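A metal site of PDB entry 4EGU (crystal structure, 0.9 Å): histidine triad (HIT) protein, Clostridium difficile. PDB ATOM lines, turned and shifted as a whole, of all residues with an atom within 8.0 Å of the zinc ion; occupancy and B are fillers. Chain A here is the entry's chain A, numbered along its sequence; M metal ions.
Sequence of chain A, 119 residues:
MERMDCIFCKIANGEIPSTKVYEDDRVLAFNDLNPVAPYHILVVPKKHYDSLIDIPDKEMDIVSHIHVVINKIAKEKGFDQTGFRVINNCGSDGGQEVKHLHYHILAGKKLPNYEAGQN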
ATOM      1  N   GLU A   2      28.800  24.558 -13.386  1.00  0.00           N
ATOM      2  CA  GLU A   2      30.078  23.992 -12.981  1.00  0.00           C
ATOM      3  C   GLU A   2      30.851  24.965 -12.099  1.00  0.00           C
ATOM      4  O   GLU A   2      30.745  26.175 -12.252  1.00  0.00           O
ATOM      5  CB  GLU A   2      30.924  23.641 -14.207  1.00  0.00           C
ATOM      6  N   ARG A   3      31.633  24.406 -11.177  1.00  0.00           N
ATOM      7  CA  ARG A   3      32.454  25.206 -10.277  1.00  0.00           C
ATOM      8  C   ARG A   3      33.902  24.718 -10.320  1.00  0.00           C
ATOM      9  O   ARG A   3      34.165  23.528 -10.181  1.00  0.00           O
ATOM     10  CB  ARG A   3      31.942  25.107  -8.847  1.00  0.00           C
ATOM     11  CG  ARG A   3      30.715  25.923  -8.537  1.00  0.00           C
ATOM     12  CD  ARG A   3      30.441  25.917  -7.037  1.00  0.00           C
ATOM     13  NE  ARG A   3      31.580  26.416  -6.275  1.00  0.00           N
ATOM     14  CZ  ARG A   3      31.578  27.558  -5.581  1.00  0.00           C
ATOM     15  NH1 ARG A   3      30.492  28.312  -5.544  1.00  0.00           N
ATOM     16  NH2 ARG A   3      32.671  27.922  -4.920  1.00  0.00           N
ATOM     17  N   MET A   4      34.832  25.636 -10.529  1.00  0.00           N
ATOM     18  CA  MET A   4      36.247  25.304 -10.589  1.00  0.00           C
ATOM     19  C   MET A   4      36.765  24.574  -9.350  1.00  0.00           C
ATOM     20  O   MET A   4      37.594  23.657  -9.453  1.00  0.00           O
ATOM     21  CB  MET A   4      37.032  26.608 -10.770  1.00  0.00           C
ATOM     22  CG  MET A   4      38.506  26.481 -10.476  1.00  0.00           C
ATOM     23  SD  MET A   4      39.486  27.954 -10.804  1.00  0.00           S
ATOM     24  CE  MET A   4      39.225  28.029 -12.562  1.00  0.00           C
ATOM     25  N   ASP A   5      36.299  24.991  -8.171  1.00  0.00           N
ATOM     26  CA  ASP A   5      36.814  24.475  -6.922  1.00  0.00           C
ATOM     27  C   ASP A   5      36.018  23.277  -6.430  1.00  0.00           C
ATOM     28  O   ASP A   5      36.233  22.820  -5.317  1.00  0.00           O
ATOM     29  CB  ASP A   5      36.869  25.565  -5.846  1.00  0.00           C
ATOM     30  CG  ASP A   5      35.520  25.975  -5.340  1.00  0.00           C
ATOM     31  OD1 ASP A   5      34.493  25.622  -5.951  1.00  0.00           O
ATOM     32  OD2 ASP A   5      35.482  26.688  -4.317  1.00  0.00           O
ATOM     33  N   CYS A   6      35.139  22.726  -7.277  1.00  0.00           N
ATOM     34  CA  CYS A   6      34.248  21.651  -6.861  1.00  0.00           C
ATOM     35  C   CYS A   6      34.763  20.290  -7.302  1.00  0.00           C
ATOM     36  O   CYS A   6      34.790  19.980  -8.479  1.00  0.00           O
ATOM     37  CB  CYS A   6      32.844  21.880  -7.420  1.00  0.00           C
ATOM     38  SG  CYS A   6      31.721  20.587  -6.844  1.00  0.00           S
ATOM     39  N   ILE A   7      35.145  19.462  -6.341  1.00  0.00           N
ATOM     40  CA  ILE A   7      35.673  18.148  -6.609  1.00  0.00           C
ATOM     41  C   ILE A   7      34.618  17.329  -7.376  1.00  0.00           C
ATOM     42  O   ILE A   7      34.965  16.582  -8.287  1.00  0.00           O
ATOM     43  CB  ILE A   7      36.083  17.414  -5.301  1.00  0.00           C
ATOM     44  CG1 ILE A   7      37.234  18.132  -4.588  1.00  0.00           C
ATOM     45  CG2 ILE A   7      36.455  15.955  -5.584  1.00  0.00           C
ATOM     46  CD1 ILE A   7      37.450  17.654  -3.168  1.00  0.00           C
ATOM     47  N   PHE A   8      33.352  17.427  -6.998  1.00  0.00           N
ATOM     48  CA  PHE A   8      32.339  16.571  -7.631  1.00  0.00           C
ATOM     49  C   PHE A   8      31.996  17.032  -9.058  1.00  0.00           C
ATOM     50  O   PHE A   8      31.667  16.179  -9.881  1.00  0.00           O
ATOM     51  CB  PHE A   8      31.090  16.412  -6.762  1.00  0.00           C
ATOM     52  CG  PHE A   8      31.295  15.586  -5.508  1.00  0.00           C
ATOM     53  CD1 PHE A   8      32.510  14.999  -5.169  1.00  0.00           C
ATOM     54  CD2 PHE A   8      30.232  15.406  -4.637  1.00  0.00           C
ATOM     55  CE1 PHE A   8      32.658  14.250  -3.994  1.00  0.00           C
ATOM     56  CE2 PHE A   8      30.381  14.665  -3.478  1.00  0.00           C
ATOM     57  CZ  PHE A   8      31.591  14.078  -3.151  1.00  0.00           C
ATOM     58  N   CYS A   9      32.092  18.320  -9.372  1.00  0.00           N
ATOM     59  CA  CYS A   9      31.967  18.736 -10.765  1.00  0.00           C
ATOM     60  C   CYS A   9      33.078  18.087 -11.595  1.00  0.00           C
ATOM     61  O   CYS A   9      32.861  17.641 -12.710  1.00  0.00           O
ATOM     62  CB  CYS A   9      32.028  20.248 -10.915  1.00  0.00           C
ATOM     63  SG  CYS A   9      30.470  21.127 -10.536  1.00  0.00           S
ATOM     64  N   LYS A  10      34.299  18.060 -11.055  1.00  0.00           N
ATOM     65  CA  LYS A  10      35.436  17.480 -11.770  1.00  0.00           C
ATOM     66  C   LYS A  10      35.294  15.953 -11.894  1.00  0.00           C
ATOM     67  O   LYS A  10      35.689  15.389 -12.911  1.00  0.00           O
ATOM     68  CB  LYS A  10      36.746  17.817 -11.074  1.00  0.00           C
ATOM     69  CG  LYS A  10      37.134  19.273 -11.014  1.00  0.00           C
ATOM     70  CD  LYS A  10      38.433  19.412 -10.222  1.00  0.00           C
ATOM     71  CE  LYS A  10      38.853  20.866 -10.014  1.00  0.00           C
ATOM     72  NZ  LYS A  10      39.223  21.567 -11.277  1.00  0.00           N
ATOM     73  N   ILE A  11      34.750  15.294 -10.870  1.00  0.00           N
ATOM     74  CA  ILE A  11      34.477  13.861 -10.941  1.00  0.00           C
ATOM     75  C   ILE A  11      33.338  13.606 -11.970  1.00  0.00           C
ATOM     76  O   ILE A  11      33.437  12.696 -12.780  1.00  0.00           O
ATOM     77  CB  ILE A  11      34.187  13.241  -9.539  1.00  0.00           C
ATOM     78  CG1 ILE A  11      35.456  13.224  -8.679  1.00  0.00           C
ATOM     79  CG2 ILE A  11      33.594  11.840  -9.685  1.00  0.00           C
ATOM     80  CD1 ILE A  11      35.275  12.706  -7.266  1.00  0.00           C
ATOM     81  N   ALA A  12      32.279  14.419 -11.942  1.00  0.00           N
ATOM     82  CA  ALA A  12      31.122  14.241 -12.843  1.00  0.00           C
ATOM     83  C   ALA A  12      31.407  14.467 -14.323  1.00  0.00           C
ATOM     84  O   ALA A  12      30.825  13.796 -15.174  1.00  0.00           O
ATOM     85  CB  ALA A  12      29.978  15.153 -12.427  1.00  0.00           C
ATOM     86  N   VAL A  44      25.381  11.547  -7.388  1.00  0.00           N
ATOM     87  CA  VAL A  44      25.396  12.999  -7.613  1.00  0.00           C
ATOM     88  C   VAL A  44      24.775  13.360  -8.948  1.00  0.00           C
ATOM     89  O   VAL A  44      24.968  12.640  -9.945  1.00  0.00           O
ATOM     90  CB  VAL A  44      26.784  13.649  -7.570  1.00  0.00           C
ATOM     91  CG1 VAL A  44      27.513  13.195  -6.342  1.00  0.00           C
ATOM     92  CG2 VAL A  44      27.598  13.334  -8.835  1.00  0.00           C
ATOM     93  N   PRO A  45      24.069  14.495  -8.997  1.00  0.00           N
ATOM     94  CA  PRO A  45      23.717  15.023 -10.301  1.00  0.00           C
ATOM     95  C   PRO A  45      24.972  15.534 -10.971  1.00  0.00           C
ATOM     96  O   PRO A  45      25.884  16.019 -10.326  1.00  0.00           O
ATOM     97  CB  PRO A  45      22.780  16.198  -9.970  1.00  0.00           C
ATOM     98  CG  PRO A  45      23.235  16.647  -8.635  1.00  0.00           C
ATOM     99  CD  PRO A  45      23.753  15.453  -7.927  1.00  0.00           C
ATOM    100  N   LYS A  46      25.000  15.460 -12.291  1.00  0.00           N
ATOM    101  CA  LYS A  46      26.054  16.118 -13.043  1.00  0.00           C
ATOM    102  C   LYS A  46      25.948  17.641 -12.927  1.00  0.00           C
ATOM    103  O   LYS A  46      26.963  18.326 -12.874  1.00  0.00           O
ATOM    104  CB  LYS A  46      26.027  15.645 -14.505  1.00  0.00           C
ATOM    105  CG  LYS A  46      26.451  14.201 -14.625  1.00  0.00           C
ATOM    106  CD  LYS A  46      26.395  13.679 -16.060  1.00  0.00           C
ATOM    107  CE  LYS A  46      27.096  12.332 -16.142  1.00  0.00           C
ATOM    108  NZ  LYS A  46      27.090  11.784 -17.508  1.00  0.00           N
ATOM    109  N   LYS A  47      24.720  18.162 -12.885  1.00  0.00           N
ATOM    110  CA  LYS A  47      24.481  19.583 -12.631  1.00  0.00           C
ATOM    111  C   LYS A  47      24.879  19.918 -11.199  1.00  0.00           C
ATOM    112  O   LYS A  47      24.563  19.176 -10.269  1.00  0.00           O
ATOM    113  CB  LYS A  47      23.005  19.931 -12.860  1.00  0.00           C
ATOM    114  CG  LYS A  47      22.643  21.382 -12.535  1.00  0.00           C
ATOM    115  CD  LYS A  47      21.204  21.733 -12.950  1.00  0.00           C
ATOM    116  CE  LYS A  47      20.803  23.147 -12.525  1.00  0.00           C
ATOM    117  NZ  LYS A  47      21.612  24.183 -13.200  1.00  0.00           N
ATOM    118  N   HIS A  48      25.548  21.035 -10.998  1.00  0.00           N
ATOM    119  CA  HIS A  48      25.924  21.491  -9.667  1.00  0.00           C
ATOM    120  C   HIS A  48      24.798  22.253  -8.979  1.00  0.00           C
ATOM    121  O   HIS A  48      24.310  23.276  -9.460  1.00  0.00           O
ATOM    122  CB  HIS A  48      27.149  22.422  -9.771  1.00  0.00           C
ATOM    123  CG  HIS A  48      27.633  22.907  -8.454  1.00  0.00           C
ATOM    124  ND1 HIS A  48      28.725  22.363  -7.804  1.00  0.00           N
ATOM    125  CD2 HIS A  48      27.133  23.863  -7.644  1.00  0.00           C
ATOM    126  CE1 HIS A  48      28.881  22.990  -6.655  1.00  0.00           C
ATOM    127  NE2 HIS A  48      27.921  23.894  -6.527  1.00  0.00           N
ATOM    128  N   TYR A  49      24.410  21.748  -7.815  1.00  0.00           N
ATOM    129  CA  TYR A  49      23.620  22.452  -6.821  1.00  0.00           C
ATOM    130  C   TYR A  49      24.448  22.463  -5.544  1.00  0.00           C
ATOM    131  O   TYR A  49      25.044  21.431  -5.195  1.00  0.00           O
ATOM    132  CB  TYR A  49      22.300  21.729  -6.503  1.00  0.00           C
ATOM    133  CG  TYR A  49      21.328  21.655  -7.620  1.00  0.00           C
ATOM    134  CD1 TYR A  49      20.460  22.720  -7.849  1.00  0.00           C
ATOM    135  CD2 TYR A  49      21.201  20.511  -8.366  1.00  0.00           C
ATOM    136  CE1 TYR A  49      19.508  22.655  -8.826  1.00  0.00           C
ATOM    137  CE2 TYR A  49      20.265  20.436  -9.359  1.00  0.00           C
ATOM    138  CZ  TYR A  49      19.417  21.513  -9.581  1.00  0.00           C
ATOM    139  OH  TYR A  49      18.468  21.420 -10.576  1.00  0.00           O
ATOM    140  N   ASP A  50      24.492  23.570  -4.810  1.00  0.00           N
ATOM    141  CA  ASP A  50      25.354  23.614  -3.655  1.00  0.00           C
ATOM    142  C   ASP A  50      24.899  22.635  -2.552  1.00  0.00           C
ATOM    143  O   ASP A  50      25.721  22.125  -1.807  1.00  0.00           O
ATOM    144  CB  ASP A  50      25.393  25.023  -3.035  1.00  0.00           C
ATOM    145  CG  ASP A  50      26.066  26.082  -3.897  1.00  0.00           C
ATOM    146  OD1 ASP A  50      26.800  25.754  -4.834  1.00  0.00           O
ATOM    147  OD2 ASP A  50      25.866  27.275  -3.593  1.00  0.00           O
ATOM    148  N   VAL A  98      31.563  18.621   1.030  1.00  0.00           N
ATOM    149  CA  VAL A  98      31.600  18.891  -0.417  1.00  0.00           C
ATOM    150  C   VAL A  98      30.269  19.506  -0.813  1.00  0.00           C
ATOM    151  O   VAL A  98      29.219  18.855  -0.702  1.00  0.00           O
ATOM    152  CB  VAL A  98      31.871  17.649  -1.248  1.00  0.00           C
ATOM    153  CG1 VAL A  98      31.858  17.982  -2.717  1.00  0.00           C
ATOM    154  CG2 VAL A  98      33.222  17.029  -0.846  1.00  0.00           C
ATOM    155  N   LYS A  99      30.333  20.749  -1.269  1.00  0.00           N
ATOM    156  CA  LYS A  99      29.136  21.546  -1.522  1.00  0.00           C
ATOM    157  C   LYS A  99      28.663  21.354  -2.969  1.00  0.00           C
ATOM    158  O   LYS A  99      28.585  22.306  -3.763  1.00  0.00           O
ATOM    159  CB  LYS A  99      29.395  23.017  -1.158  1.00  0.00           C
ATOM    160  CG  LYS A  99      29.620  23.230   0.337  1.00  0.00           C
ATOM    161  CD  LYS A  99      29.893  24.693   0.648  1.00  0.00           C
ATOM    162  CE  LYS A  99      30.198  24.929   2.117  1.00  0.00           C
ATOM    163  NZ  LYS A  99      30.481  26.370   2.407  1.00  0.00           N
ATOM    164  N   HIS A 100      28.323  20.119  -3.264  1.00  0.00           N
ATOM    165  CA  HIS A 100      27.709  19.693  -4.529  1.00  0.00           C
ATOM    166  C   HIS A 100      26.736  18.593  -4.133  1.00  0.00           C
ATOM    167  O   HIS A 100      27.183  17.596  -3.555  1.00  0.00           O
ATOM    168  CB  HIS A 100      28.776  19.157  -5.505  1.00  0.00           C
ATOM    169  CG  HIS A 100      28.248  18.675  -6.818  1.00  0.00           C
ATOM    170  ND1 HIS A 100      28.710  19.191  -8.014  1.00  0.00           N
ATOM    171  CD2 HIS A 100      27.387  17.671  -7.114  1.00  0.00           C
ATOM    172  CE1 HIS A 100      28.123  18.529  -9.001  1.00  0.00           C
ATOM    173  NE2 HIS A 100      27.335  17.590  -8.477  1.00  0.00           N
ATOM    174  N   LEU A 101      25.444  18.768  -4.420  1.00  0.00           N
ATOM    175  CA  LEU A 101      24.419  17.802  -3.995  1.00  0.00           C
ATOM    176  C   LEU A 101      24.886  16.376  -4.179  1.00  0.00           C
ATOM    177  O   LEU A 101      25.278  15.938  -5.273  1.00  0.00           O
ATOM    178  CB  LEU A 101      23.126  17.966  -4.806  1.00  0.00           C
ATOM    179  CG  LEU A 101      21.941  17.148  -4.281  1.00  0.00           C
ATOM    180  CD1 LEU A 101      21.376  17.762  -2.988  1.00  0.00           C
ATOM    181  CD2 LEU A 101      20.893  17.014  -5.336  1.00  0.00           C
HETATM  182 ZN    ZN M   1      29.968  20.826  -8.332  1.00  0.00          ZN
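SG of Cys 6 lies close to N of Phe 8, at 3.6 Å. A ring nitrogen (NE2) of His 48 sits close to the backbone carbonyl oxygen (O) of Lys 99 (3.3 Å). The side-chain sulfur (SG) of Cys 9 lies close to the backbone NH (N) of Arg 3 (3.5 Å). A ring nitrogen (NE2) of His 48 sits at hydrogen-bond distance from the side-chain carboxylate (OD1) of Asp 50, 2.8 Å away. The backbone carbonyl oxygen of Pro 45 sits at hydrogen-bond distance from a ring nitrogen (NE2) of His 100 (2.8 Å).
Of the 22 residues printed, 4 come within 4 Å of the zinc ion. The nearest printed residue that does not touch the zinc ion is Phe 8 (4.4 Å).
ND1 of His 48 is bound to the zinc ion (2.0 Å). A ring nitrogen (ND1) of His 100 is bound to the zinc ion. SG of Cys 9 binds the zinc ion (2.3 Å). The zinc ion is bound by the side-chain sulfur (SG) of Cys 6, at 2.3 Å. The zinc ion has four donor atoms within binding distance.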
